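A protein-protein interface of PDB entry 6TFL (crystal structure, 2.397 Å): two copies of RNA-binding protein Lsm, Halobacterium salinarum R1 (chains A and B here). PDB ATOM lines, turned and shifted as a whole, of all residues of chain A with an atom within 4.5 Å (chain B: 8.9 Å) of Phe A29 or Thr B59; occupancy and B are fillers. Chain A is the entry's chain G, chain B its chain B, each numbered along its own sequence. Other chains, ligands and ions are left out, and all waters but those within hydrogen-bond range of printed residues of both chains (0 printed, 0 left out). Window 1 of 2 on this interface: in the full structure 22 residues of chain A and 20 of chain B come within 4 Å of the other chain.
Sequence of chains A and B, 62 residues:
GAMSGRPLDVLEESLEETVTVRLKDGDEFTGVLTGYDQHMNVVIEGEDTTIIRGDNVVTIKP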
ATOM      1  N   VAL A  19       8.765 -24.896  17.039  1.00  0.00           N
ATOM      2  CA  VAL A  19       7.650 -24.243  16.354  1.00  0.00           C
ATOM      3  C   VAL A  19       7.796 -24.491  14.860  1.00  0.00           C
ATOM      4  O   VAL A  19       8.785 -25.071  14.400  1.00  0.00           O
ATOM      5  CB  VAL A  19       7.587 -22.726  16.636  1.00  0.00           C
ATOM      6  CG1 VAL A  19       7.575 -22.452  18.130  1.00  0.00           C
ATOM      7  CG2 VAL A  19       8.755 -22.009  15.948  1.00  0.00           C
ATOM      8  N   THR A  20       6.810 -24.032  14.089  1.00  0.00           N
ATOM      9  CA  THR A  20       6.825 -24.157  12.634  1.00  0.00           C
ATOM     10  C   THR A  20       6.405 -22.835  12.009  1.00  0.00           C
ATOM     11  O   THR A  20       5.308 -22.338  12.280  1.00  0.00           O
ATOM     12  CB  THR A  20       5.909 -25.292  12.164  1.00  0.00           C
ATOM     13  OG1 THR A  20       6.461 -26.535  12.602  1.00  0.00           O
ATOM     14  CG2 THR A  20       5.811 -25.306  10.640  1.00  0.00           C
ATOM     15  N   VAL A  21       7.279 -22.269  11.183  1.00  0.00           N
ATOM     16  CA  VAL A  21       7.047 -20.993  10.508  1.00  0.00           C
ATOM     17  C   VAL A  21       6.729 -21.259   9.036  1.00  0.00           C
ATOM     18  O   VAL A  21       7.447 -22.011   8.367  1.00  0.00           O
ATOM     19  CB  VAL A  21       8.271 -20.072  10.659  1.00  0.00           C
ATOM     20  CG1 VAL A  21       7.963 -18.672  10.185  1.00  0.00           C
ATOM     21  CG2 VAL A  21       8.723 -20.049  12.118  1.00  0.00           C
ATOM     22  N   LEU A  23       6.157 -19.356   5.286  1.00  0.00           N
ATOM     23  CA  LEU A  23       6.499 -18.115   4.594  1.00  0.00           C
ATOM     24  C   LEU A  23       5.568 -17.851   3.411  1.00  0.00           C
ATOM     25  O   LEU A  23       4.837 -18.735   2.953  1.00  0.00           O
ATOM     26  CB  LEU A  23       7.951 -18.150   4.114  1.00  0.00           C
ATOM     27  CG  LEU A  23       9.014 -18.430   5.175  1.00  0.00           C
ATOM     28  CD1 LEU A  23      10.407 -18.226   4.617  1.00  0.00           C
ATOM     29  CD2 LEU A  23       8.782 -17.542   6.377  1.00  0.00           C
ATOM     30  N   ASP A  27       7.444 -21.881   1.767  1.00  0.00           N
ATOM     31  CA  ASP A  27       8.400 -22.675   2.525  1.00  0.00           C
ATOM     32  C   ASP A  27       8.003 -22.759   3.992  1.00  0.00           C
ATOM     33  O   ASP A  27       7.362 -21.859   4.539  1.00  0.00           O
ATOM     34  CB  ASP A  27       9.805 -22.081   2.423  1.00  0.00           C
ATOM     35  CG  ASP A  27      10.528 -22.526   1.183  1.00  0.00           C
ATOM     36  OD1 ASP A  27       9.876 -23.163   0.327  1.00  0.00           O
ATOM     37  OD2 ASP A  27      11.740 -22.231   1.058  1.00  0.00           O
ATOM     38  N   GLU A  28       8.416 -23.849   4.635  1.00  0.00           N
ATOM     39  CA  GLU A  28       8.123 -24.077   6.040  1.00  0.00           C
ATOM     40  C   GLU A  28       9.406 -24.432   6.768  1.00  0.00           C
ATOM     41  O   GLU A  28      10.219 -25.219   6.275  1.00  0.00           O
ATOM     42  CB  GLU A  28       7.092 -25.188   6.237  1.00  0.00           C
ATOM     43  CG  GLU A  28       5.664 -24.768   5.939  1.00  0.00           C
ATOM     44  CD  GLU A  28       4.641 -25.740   6.512  1.00  0.00           C
ATOM     45  OE1 GLU A  28       3.430 -25.545   6.269  1.00  0.00           O
ATOM     46  OE2 GLU A  28       5.052 -26.697   7.207  1.00  0.00           O
ATOM     47  N   PHE A  29       9.579 -23.844   7.944  1.00  0.00           N
ATOM     48  CA  PHE A  29      10.766 -24.050   8.752  1.00  0.00           C
ATOM     49  C   PHE A  29      10.320 -24.577  10.101  1.00  0.00           C
ATOM     50  O   PHE A  29       9.492 -23.952  10.769  1.00  0.00           O
ATOM     51  CB  PHE A  29      11.552 -22.750   8.896  1.00  0.00           C
ATOM     52  CG  PHE A  29      12.225 -22.328   7.643  1.00  0.00           C
ATOM     53  CD1 PHE A  29      11.532 -21.625   6.673  1.00  0.00           C
ATOM     54  CD2 PHE A  29      13.551 -22.650   7.407  1.00  0.00           C
ATOM     55  CE1 PHE A  29      12.157 -21.233   5.500  1.00  0.00           C
ATOM     56  CE2 PHE A  29      14.173 -22.248   6.231  1.00  0.00           C
ATOM     57  CZ  PHE A  29      13.463 -21.553   5.282  1.00  0.00           C
ATOM     58  N   THR A  30      10.833 -25.740  10.483  1.00  0.00           N
ATOM     59  CA  THR A  30      10.533 -26.327  11.777  1.00  0.00           C
ATOM     60  C   THR A  30      11.819 -26.433  12.572  1.00  0.00           C
ATOM     61  O   THR A  30      12.837 -26.914  12.066  1.00  0.00           O
ATOM     62  CB  THR A  30       9.869 -27.693  11.635  1.00  0.00           C
ATOM     63  OG1 THR A  30       8.620 -27.514  10.966  1.00  0.00           O
ATOM     64  CG2 THR A  30       9.620 -28.308  13.022  1.00  0.00           C
ATOM     65  N   GLY A  31      11.774 -25.964  13.808  1.00  0.00           N
ATOM     66  CA  GLY A  31      12.939 -26.017  14.661  1.00  0.00           C
ATOM     67  C   GLY A  31      12.652 -25.273  15.943  1.00  0.00           C
ATOM     68  O   GLY A  31      11.530 -24.815  16.175  1.00  0.00           O
ATOM     69  N   THR A  50      18.688 -20.686  11.380  1.00  0.00           N
ATOM     70  CA  THR A  50      18.085 -19.862  10.333  1.00  0.00           C
ATOM     71  C   THR A  50      17.503 -18.610  10.970  1.00  0.00           C
ATOM     72  O   THR A  50      16.705 -18.705  11.912  1.00  0.00           O
ATOM     73  CB  THR A  50      16.981 -20.597   9.553  1.00  0.00           C
ATOM     74  OG1 THR A  50      17.455 -21.861   9.071  1.00  0.00           O
ATOM     75  CG2 THR A  50      16.530 -19.741   8.368  1.00  0.00           C
ATOM     76  N   ILE A  51      17.910 -17.446  10.468  1.00  0.00           N
ATOM     77  CA  ILE A  51      17.218 -16.197  10.748  1.00  0.00           C
ATOM     78  C   ILE A  51      16.202 -15.970   9.644  1.00  0.00           C
ATOM     79  O   ILE A  51      16.530 -16.062   8.453  1.00  0.00           O
ATOM     80  CB  ILE A  51      18.197 -15.018  10.840  1.00  0.00           C
ATOM     81  CG1 ILE A  51      19.308 -15.318  11.844  1.00  0.00           C
ATOM     82  CG2 ILE A  51      17.460 -13.761  11.252  1.00  0.00           C
ATOM     83  CD1 ILE A  51      20.330 -14.184  11.965  1.00  0.00           C
ATOM     84  N   ILE A  52      14.966 -15.683  10.029  1.00  0.00           N
ATOM     85  CA  ILE A  52      13.887 -15.415   9.089  1.00  0.00           C
ATOM     86  C   ILE A  52      13.438 -13.979   9.293  1.00  0.00           C
ATOM     87  O   ILE A  52      13.155 -13.564  10.425  1.00  0.00           O
ATOM     88  CB  ILE A  52      12.716 -16.393   9.286  1.00  0.00           C
ATOM     89  CG1 ILE A  52      13.185 -17.815   9.014  1.00  0.00           C
ATOM     90  CG2 ILE A  52      11.580 -16.037   8.372  1.00  0.00           C
ATOM     91  CD1 ILE A  52      12.189 -18.849   9.394  1.00  0.00           C
ATOM     92  N   LEU B  11      23.028 -11.857  14.468  1.00  0.00           N
ATOM     93  CA  LEU B  11      23.826 -11.213  13.425  1.00  0.00           C
ATOM     94  C   LEU B  11      25.094 -10.590  14.003  1.00  0.00           C
ATOM     95  O   LEU B  11      26.173 -10.734  13.428  1.00  0.00           O
ATOM     96  CB  LEU B  11      22.995 -10.157  12.697  1.00  0.00           C
ATOM     97  CG  LEU B  11      21.978 -10.667  11.661  1.00  0.00           C
ATOM     98  CD1 LEU B  11      21.330  -9.496  10.930  1.00  0.00           C
ATOM     99  CD2 LEU B  11      22.622 -11.633  10.677  1.00  0.00           C
ATOM    100  N   VAL B  19      28.278 -16.106   6.138  1.00  0.00           N
ATOM    101  CA  VAL B  19      26.849 -16.379   6.169  1.00  0.00           C
ATOM    102  C   VAL B  19      26.367 -16.543   4.732  1.00  0.00           C
ATOM    103  O   VAL B  19      27.054 -16.181   3.770  1.00  0.00           O
ATOM    104  CB  VAL B  19      26.043 -15.278   6.898  1.00  0.00           C
ATOM    105  CG1 VAL B  19      26.681 -14.922   8.246  1.00  0.00           C
ATOM    106  CG2 VAL B  19      25.944 -14.042   6.036  1.00  0.00           C
ATOM    107  N   THR B  20      25.169 -17.099   4.597  1.00  0.00           N
ATOM    108  CA  THR B  20      24.460 -17.172   3.329  1.00  0.00           C
ATOM    109  C   THR B  20      23.142 -16.424   3.458  1.00  0.00           C
ATOM    110  O   THR B  20      22.364 -16.683   4.389  1.00  0.00           O
ATOM    111  CB  THR B  20      24.211 -18.621   2.917  1.00  0.00           C
ATOM    112  OG1 THR B  20      25.475 -19.243   2.643  1.00  0.00           O
ATOM    113  CG2 THR B  20      23.326 -18.679   1.648  1.00  0.00           C
ATOM    114  N   VAL B  21      22.900 -15.506   2.521  1.00  0.00           N
ATOM    115  CA  VAL B  21      21.724 -14.639   2.519  1.00  0.00           C
ATOM    116  C   VAL B  21      20.854 -15.028   1.338  1.00  0.00           C
ATOM    117  O   VAL B  21      21.315 -14.999   0.192  1.00  0.00           O
ATOM    118  CB  VAL B  21      22.122 -13.157   2.435  1.00  0.00           C
ATOM    119  CG1 VAL B  21      20.874 -12.277   2.357  1.00  0.00           C
ATOM    120  CG2 VAL B  21      23.015 -12.766   3.626  1.00  0.00           C
ATOM    121  N   ARG B  22      19.590 -15.361   1.602  1.00  0.00           N
ATOM    122  CA  ARG B  22      18.656 -15.749   0.551  1.00  0.00           C
ATOM    123  C   ARG B  22      17.613 -14.654   0.331  1.00  0.00           C
ATOM    124  O   ARG B  22      16.972 -14.196   1.286  1.00  0.00           O
ATOM    125  CB  ARG B  22      17.986 -17.070   0.903  1.00  0.00           C
ATOM    126  CG  ARG B  22      17.574 -17.879  -0.293  1.00  0.00           C
ATOM    127  CD  ARG B  22      17.049 -19.237   0.146  1.00  0.00           C
ATOM    128  NE  ARG B  22      15.600 -19.295  -0.016  1.00  0.00           N
ATOM    129  CZ  ARG B  22      14.734 -19.439   0.979  1.00  0.00           C
ATOM    130  NH1 ARG B  22      15.157 -19.562   2.233  1.00  0.00           N
ATOM    131  NH2 ARG B  22      13.440 -19.471   0.710  1.00  0.00           N
ATOM    132  N   LEU B  23      17.444 -14.236  -0.926  1.00  0.00           N
ATOM    133  CA  LEU B  23      16.580 -13.108  -1.271  1.00  0.00           C
ATOM    134  C   LEU B  23      15.262 -13.571  -1.882  1.00  0.00           C
ATOM    135  O   LEU B  23      15.153 -14.680  -2.408  1.00  0.00           O
ATOM    136  CB  LEU B  23      17.270 -12.156  -2.246  1.00  0.00           C
ATOM    137  CG  LEU B  23      18.713 -11.783  -1.931  1.00  0.00           C
ATOM    138  CD1 LEU B  23      19.166 -10.669  -2.847  1.00  0.00           C
ATOM    139  CD2 LEU B  23      18.830 -11.366  -0.488  1.00  0.00           C
ATOM    140  N   LYS B  24      14.265 -12.677  -1.830  1.00  0.00           N
ATOM    141  CA  LYS B  24      12.930 -12.992  -2.343  1.00  0.00           C
ATOM    142  C   LYS B  24      12.945 -13.425  -3.805  1.00  0.00           C
ATOM    143  O   LYS B  24      12.061 -14.183  -4.226  1.00  0.00           O
ATOM    144  CB  LYS B  24      11.990 -11.798  -2.178  1.00  0.00           C
ATOM    145  CG  LYS B  24      11.626 -11.459  -0.742  1.00  0.00           C
ATOM    146  CD  LYS B  24      10.684 -10.252  -0.704  1.00  0.00           C
ATOM    147  CE  LYS B  24      10.089 -10.035   0.695  1.00  0.00           C
ATOM    148  NZ  LYS B  24      11.162  -9.850   1.730  1.00  0.00           N
ATOM    149  N   ASP B  27      17.844 -15.489  -5.427  1.00  0.00           N
ATOM    150  CA  ASP B  27      19.298 -15.450  -5.405  1.00  0.00           C
ATOM    151  C   ASP B  27      19.820 -15.661  -3.990  1.00  0.00           C
ATOM    152  O   ASP B  27      19.182 -15.291  -3.001  1.00  0.00           O
ATOM    153  CB  ASP B  27      19.823 -14.122  -5.954  1.00  0.00           C
ATOM    154  CG  ASP B  27      19.553 -13.948  -7.448  1.00  0.00           C
ATOM    155  OD1 ASP B  27      19.341 -14.962  -8.151  1.00  0.00           O
ATOM    156  OD2 ASP B  27      19.555 -12.788  -7.916  1.00  0.00           O
ATOM    157  N   GLU B  28      20.992 -16.274  -3.906  1.00  0.00           N
ATOM    158  CA  GLU B  28      21.694 -16.482  -2.654  1.00  0.00           C
ATOM    159  C   GLU B  28      23.028 -15.766  -2.727  1.00  0.00           C
ATOM    160  O   GLU B  28      23.677 -15.766  -3.769  1.00  0.00           O
ATOM    161  CB  GLU B  28      21.935 -17.962  -2.390  1.00  0.00           C
ATOM    162  CG  GLU B  28      20.681 -18.786  -2.203  1.00  0.00           C
ATOM    163  CD  GLU B  28      20.993 -20.131  -1.564  1.00  0.00           C
ATOM    164  OE1 GLU B  28      22.181 -20.354  -1.221  1.00  0.00           O
ATOM    165  OE2 GLU B  28      20.063 -20.953  -1.397  1.00  0.00           O
ATOM    166  N   PHE B  29      23.449 -15.176  -1.615  1.00  0.00           N
ATOM    167  CA  PHE B  29      24.755 -14.551  -1.506  1.00  0.00           C
ATOM    168  C   PHE B  29      25.480 -15.165  -0.326  1.00  0.00           C
ATOM    169  O   PHE B  29      24.937 -15.203   0.780  1.00  0.00           O
ATOM    170  CB  PHE B  29      24.632 -13.039  -1.331  1.00  0.00           C
ATOM    171  CG  PHE B  29      24.200 -12.326  -2.584  1.00  0.00           C
ATOM    172  CD1 PHE B  29      22.858 -12.281  -2.943  1.00  0.00           C
ATOM    173  CD2 PHE B  29      25.134 -11.708  -3.411  1.00  0.00           C
ATOM    174  CE1 PHE B  29      22.453 -11.627  -4.106  1.00  0.00           C
ATOM    175  CE2 PHE B  29      24.735 -11.049  -4.570  1.00  0.00           C
ATOM    176  CZ  PHE B  29      23.388 -11.013  -4.921  1.00  0.00           C
ATOM    177  N   MET B  40      18.042  -4.792   8.916  1.00  0.00           N
ATOM    178  CA  MET B  40      18.633  -5.995   8.336  1.00  0.00           C
ATOM    179  C   MET B  40      19.226  -5.750   6.944  1.00  0.00           C
ATOM    180  O   MET B  40      19.307  -6.669   6.127  1.00  0.00           O
ATOM    181  CB  MET B  40      17.640  -7.163   8.287  1.00  0.00           C
ATOM    182  CG  MET B  40      18.301  -8.525   8.465  1.00  0.00           C
ATOM    183  SD  MET B  40      17.148  -9.883   8.769  1.00  0.00           S
ATOM    184  CE  MET B  40      16.547  -9.443  10.401  1.00  0.00           C
ATOM    185  N   VAL B  42      22.554  -5.796   5.046  1.00  0.00           N
ATOM    186  CA  VAL B  42      23.765  -6.534   5.363  1.00  0.00           C
ATOM    187  C   VAL B  42      24.849  -6.179   4.355  1.00  0.00           C
ATOM    188  O   VAL B  42      24.568  -5.822   3.206  1.00  0.00           O
ATOM    189  CB  VAL B  42      23.505  -8.061   5.408  1.00  0.00           C
ATOM    190  CG1 VAL B  42      22.566  -8.384   6.534  1.00  0.00           C
ATOM    191  CG2 VAL B  42      22.908  -8.553   4.112  1.00  0.00           C
ATOM    192  N   ILE B  52      23.389  -5.530   0.615  1.00  0.00           N
ATOM    193  CA  ILE B  52      22.066  -6.072   0.330  1.00  0.00           C
ATOM    194  C   ILE B  52      21.052  -5.304   1.160  1.00  0.00           C
ATOM    195  O   ILE B  52      21.179  -5.224   2.390  1.00  0.00           O
ATOM    196  CB  ILE B  52      21.975  -7.572   0.664  1.00  0.00           C
ATOM    197  CG1 ILE B  52      23.049  -8.380  -0.064  1.00  0.00           C
ATOM    198  CG2 ILE B  52      20.560  -8.101   0.374  1.00  0.00           C
ATOM    199  CD1 ILE B  52      22.969  -9.876   0.244  1.00  0.00           C
ATOM    200  N   GLY B  54      17.707  -4.797   3.183  1.00  0.00           N
ATOM    201  CA  GLY B  54      17.087  -5.797   4.045  1.00  0.00           C
ATOM    202  C   GLY B  54      15.723  -6.282   3.576  1.00  0.00           C
ATOM    203  O   GLY B  54      15.379  -7.454   3.756  1.00  0.00           O
ATOM    204  N   ASN B  56      14.735  -7.124   0.833  1.00  0.00           N
ATOM    205  CA  ASN B  56      14.839  -8.224  -0.116  1.00  0.00           C
ATOM    206  C   ASN B  56      15.090  -9.571   0.554  1.00  0.00           C
ATOM    207  O   ASN B  56      14.969 -10.608  -0.110  1.00  0.00           O
ATOM    208  CB  ASN B  56      15.974  -7.970  -1.119  1.00  0.00           C
ATOM    209  CG  ASN B  56      15.863  -6.625  -1.809  1.00  0.00           C
ATOM    210  OD1 ASN B  56      15.158  -6.488  -2.805  1.00  0.00           O
ATOM    211  ND2 ASN B  56      16.555  -5.625  -1.277  1.00  0.00           N
ATOM    212  N   VAL B  57      15.431  -9.581   1.839  1.00  0.00           N
ATOM    213  CA  VAL B  57      15.956 -10.775   2.492  1.00  0.00           C
ATOM    214  C   VAL B  57      14.809 -11.688   2.921  1.00  0.00           C
ATOM    215  O   VAL B  57      13.840 -11.246   3.553  1.00  0.00           O
ATOM    216  CB  VAL B  57      16.829 -10.374   3.695  1.00  0.00           C
ATOM    217  CG1 VAL B  57      17.303 -11.599   4.466  1.00  0.00           C
ATOM    218  CG2 VAL B  57      18.002  -9.493   3.239  1.00  0.00           C
ATOM    219  N   VAL B  58      14.910 -12.969   2.580  1.00  0.00           N
ATOM    220  CA  VAL B  58      14.011 -13.972   3.146  1.00  0.00           C
ATOM    221  C   VAL B  58      14.652 -14.585   4.392  1.00  0.00           C
ATOM    222  O   VAL B  58      14.182 -14.371   5.516  1.00  0.00           O
ATOM    223  CB  VAL B  58      13.664 -15.052   2.107  1.00  0.00           C
ATOM    224  CG1 VAL B  58      12.739 -16.100   2.709  1.00  0.00           C
ATOM    225  CG2 VAL B  58      13.032 -14.413   0.917  1.00  0.00           C
ATOM    226  N   THR B  59      15.733 -15.343   4.211  1.00  0.00           N
ATOM    227  CA  THR B  59      16.446 -15.960   5.321  1.00  0.00           C
ATOM    228  C   THR B  59      17.916 -15.570   5.293  1.00  0.00           C
ATOM    229  O   THR B  59      18.468 -15.219   4.242  1.00  0.00           O
ATOM    230  CB  THR B  59      16.339 -17.497   5.299  1.00  0.00           C
ATOM    231  OG1 THR B  59      16.905 -17.992   4.081  1.00  0.00           O
ATOM    232  CG2 THR B  59      14.879 -17.954   5.391  1.00  0.00           C
ATOM    233  N   ILE B  60      18.536 -15.627   6.473  1.00  0.00           N
ATOM    234  CA  ILE B  60      19.980 -15.582   6.644  1.00  0.00           C
ATOM    235  C   ILE B  60      20.395 -16.832   7.415  1.00  0.00           C
ATOM    236  O   ILE B  60      19.867 -17.102   8.503  1.00  0.00           O
ATOM    237  CB  ILE B  60      20.432 -14.318   7.388  1.00  0.00           C
ATOM    238  CG1 ILE B  60      19.985 -13.068   6.624  1.00  0.00           C
ATOM    239  CG2 ILE B  60      21.952 -14.369   7.631  1.00  0.00           C
ATOM    240  CD1 ILE B  60      20.470 -11.753   7.185  1.00  0.00           C
ATOM    241  N   LYS B  61      21.325 -17.599   6.855  1.00  0.00           N
ATOM    242  CA  LYS B  61      21.881 -18.750   7.554  1.00  0.00           C
ATOM    243  C   LYS B  61      23.267 -18.394   8.086  1.00  0.00           C
ATOM    244  O   LYS B  61      24.265 -18.507   7.361  1.00  0.00           O
ATOM    245  CB  LYS B  61      21.935 -19.962   6.630  1.00  0.00           C
ATOM    246  CG  LYS B  61      20.542 -20.464   6.241  1.00  0.00           C
ATOM    247  CD  LYS B  61      20.594 -21.863   5.640  1.00  0.00           C
ATOM    248  CE  LYS B  61      19.583 -22.791   6.292  1.00  0.00           C
ATOM    249  NZ  LYS B  61      19.799 -22.947   7.773  1.00  0.00           N
ATOM    250  N   PRO B  62      23.366 -17.934   9.343  1.00  0.00           N
ATOM    251  CA  PRO B  62      24.625 -17.464   9.919  1.00  0.00           C
ATOM    252  C   PRO B  62      25.522 -18.621  10.347  1.00  0.00           C
ATOM    253  O   PRO B  62      25.035 -19.724  10.626  1.00  0.00           O
ATOM    254  CB  PRO B  62      24.166 -16.654  11.129  1.00  0.00           C
ATOM    255  CG  PRO B  62      22.915 -17.366  11.584  1.00  0.00           C
ATOM    256  CD  PRO B  62      22.261 -17.890  10.324  1.00  0.00           C
ATOM    257  OXT PRO B  62      26.747 -18.475  10.424  1.00  0.00           O
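The side-chain amino group (NZ) of Lys B61 sits at hydrogen-bond distance from the side-chain hydroxyl (OG1) of Thr A50 (2.9 Å). The backbone carbonyl oxygen (O) of Ile B60 is in hydrogen-bond range of the backbone NH (N) of Ile A51 (2.8 Å). NH2 of Arg B22 lies within salt-bridge range of OD2 of Asp A27 (3.3 Å).
O of Arg B22 sits at hydrogen-bond distance from N of Val B58 (2.7 Å). The backbone NH of Val A21 lies within hydrogen-bond range of the backbone carbonyl oxygen of Phe A29 (2.8 Å). The backbone carbonyl oxygen (O) of Thr B20 lies within hydrogen-bond range of the backbone NH (N) of Lys B61 (2.8 Å). The backbone NH of Arg B22 sits at hydrogen-bond distance from the backbone carbonyl oxygen of Thr B59 (2.9 Å).
Among the printed residues, merely in contact across the chains: Leu A23 with Val B58, Phe A29 with Thr B59, Thr A50 with Thr B59, Thr A50 with Ile B60, Ile A51 with Leu B11, Ile A51 with Thr B59 and Ile A52 with Val B58.
No residue of chain B comes within 4 Å of Thr A20. Of the printed residues of chain B, Leu A23 touches Val B58 (3.7 Å). Thr A30 touches none of the printed residues of chain B. Printed residues of chain B within 4 Å of Ile A52: Val B58 (3.7 Å). Printed residues of chain A within 4 Å of Thr B59: Phe A29, Thr A50 and Ile A51. Of the printed residues of chain A, Ile B60 touches Thr A50 and Ile A51.
Hydrophobic or aromatic side chains of chain A within 4 Å of the printed part of chain B: Leu A23, Phe A29 and Ile A51. Along chain A the printed residues that touch a printed residue of chain B span positions 23 to 52. Printed residues of chain B that touch a printed residue of chain A: Leu B11, Arg B22, Val B58, Thr B59, Ile B60 and Lys B61. Among the printed residues, 10 pairs touch across the chains.
Positions printed for both chains: 19, 20, 21, 23, 27, 28, 29 and 52. Of the 10 pairs that touch across the chains among the printed residues, none has its exchanged pair printed and touching as well.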
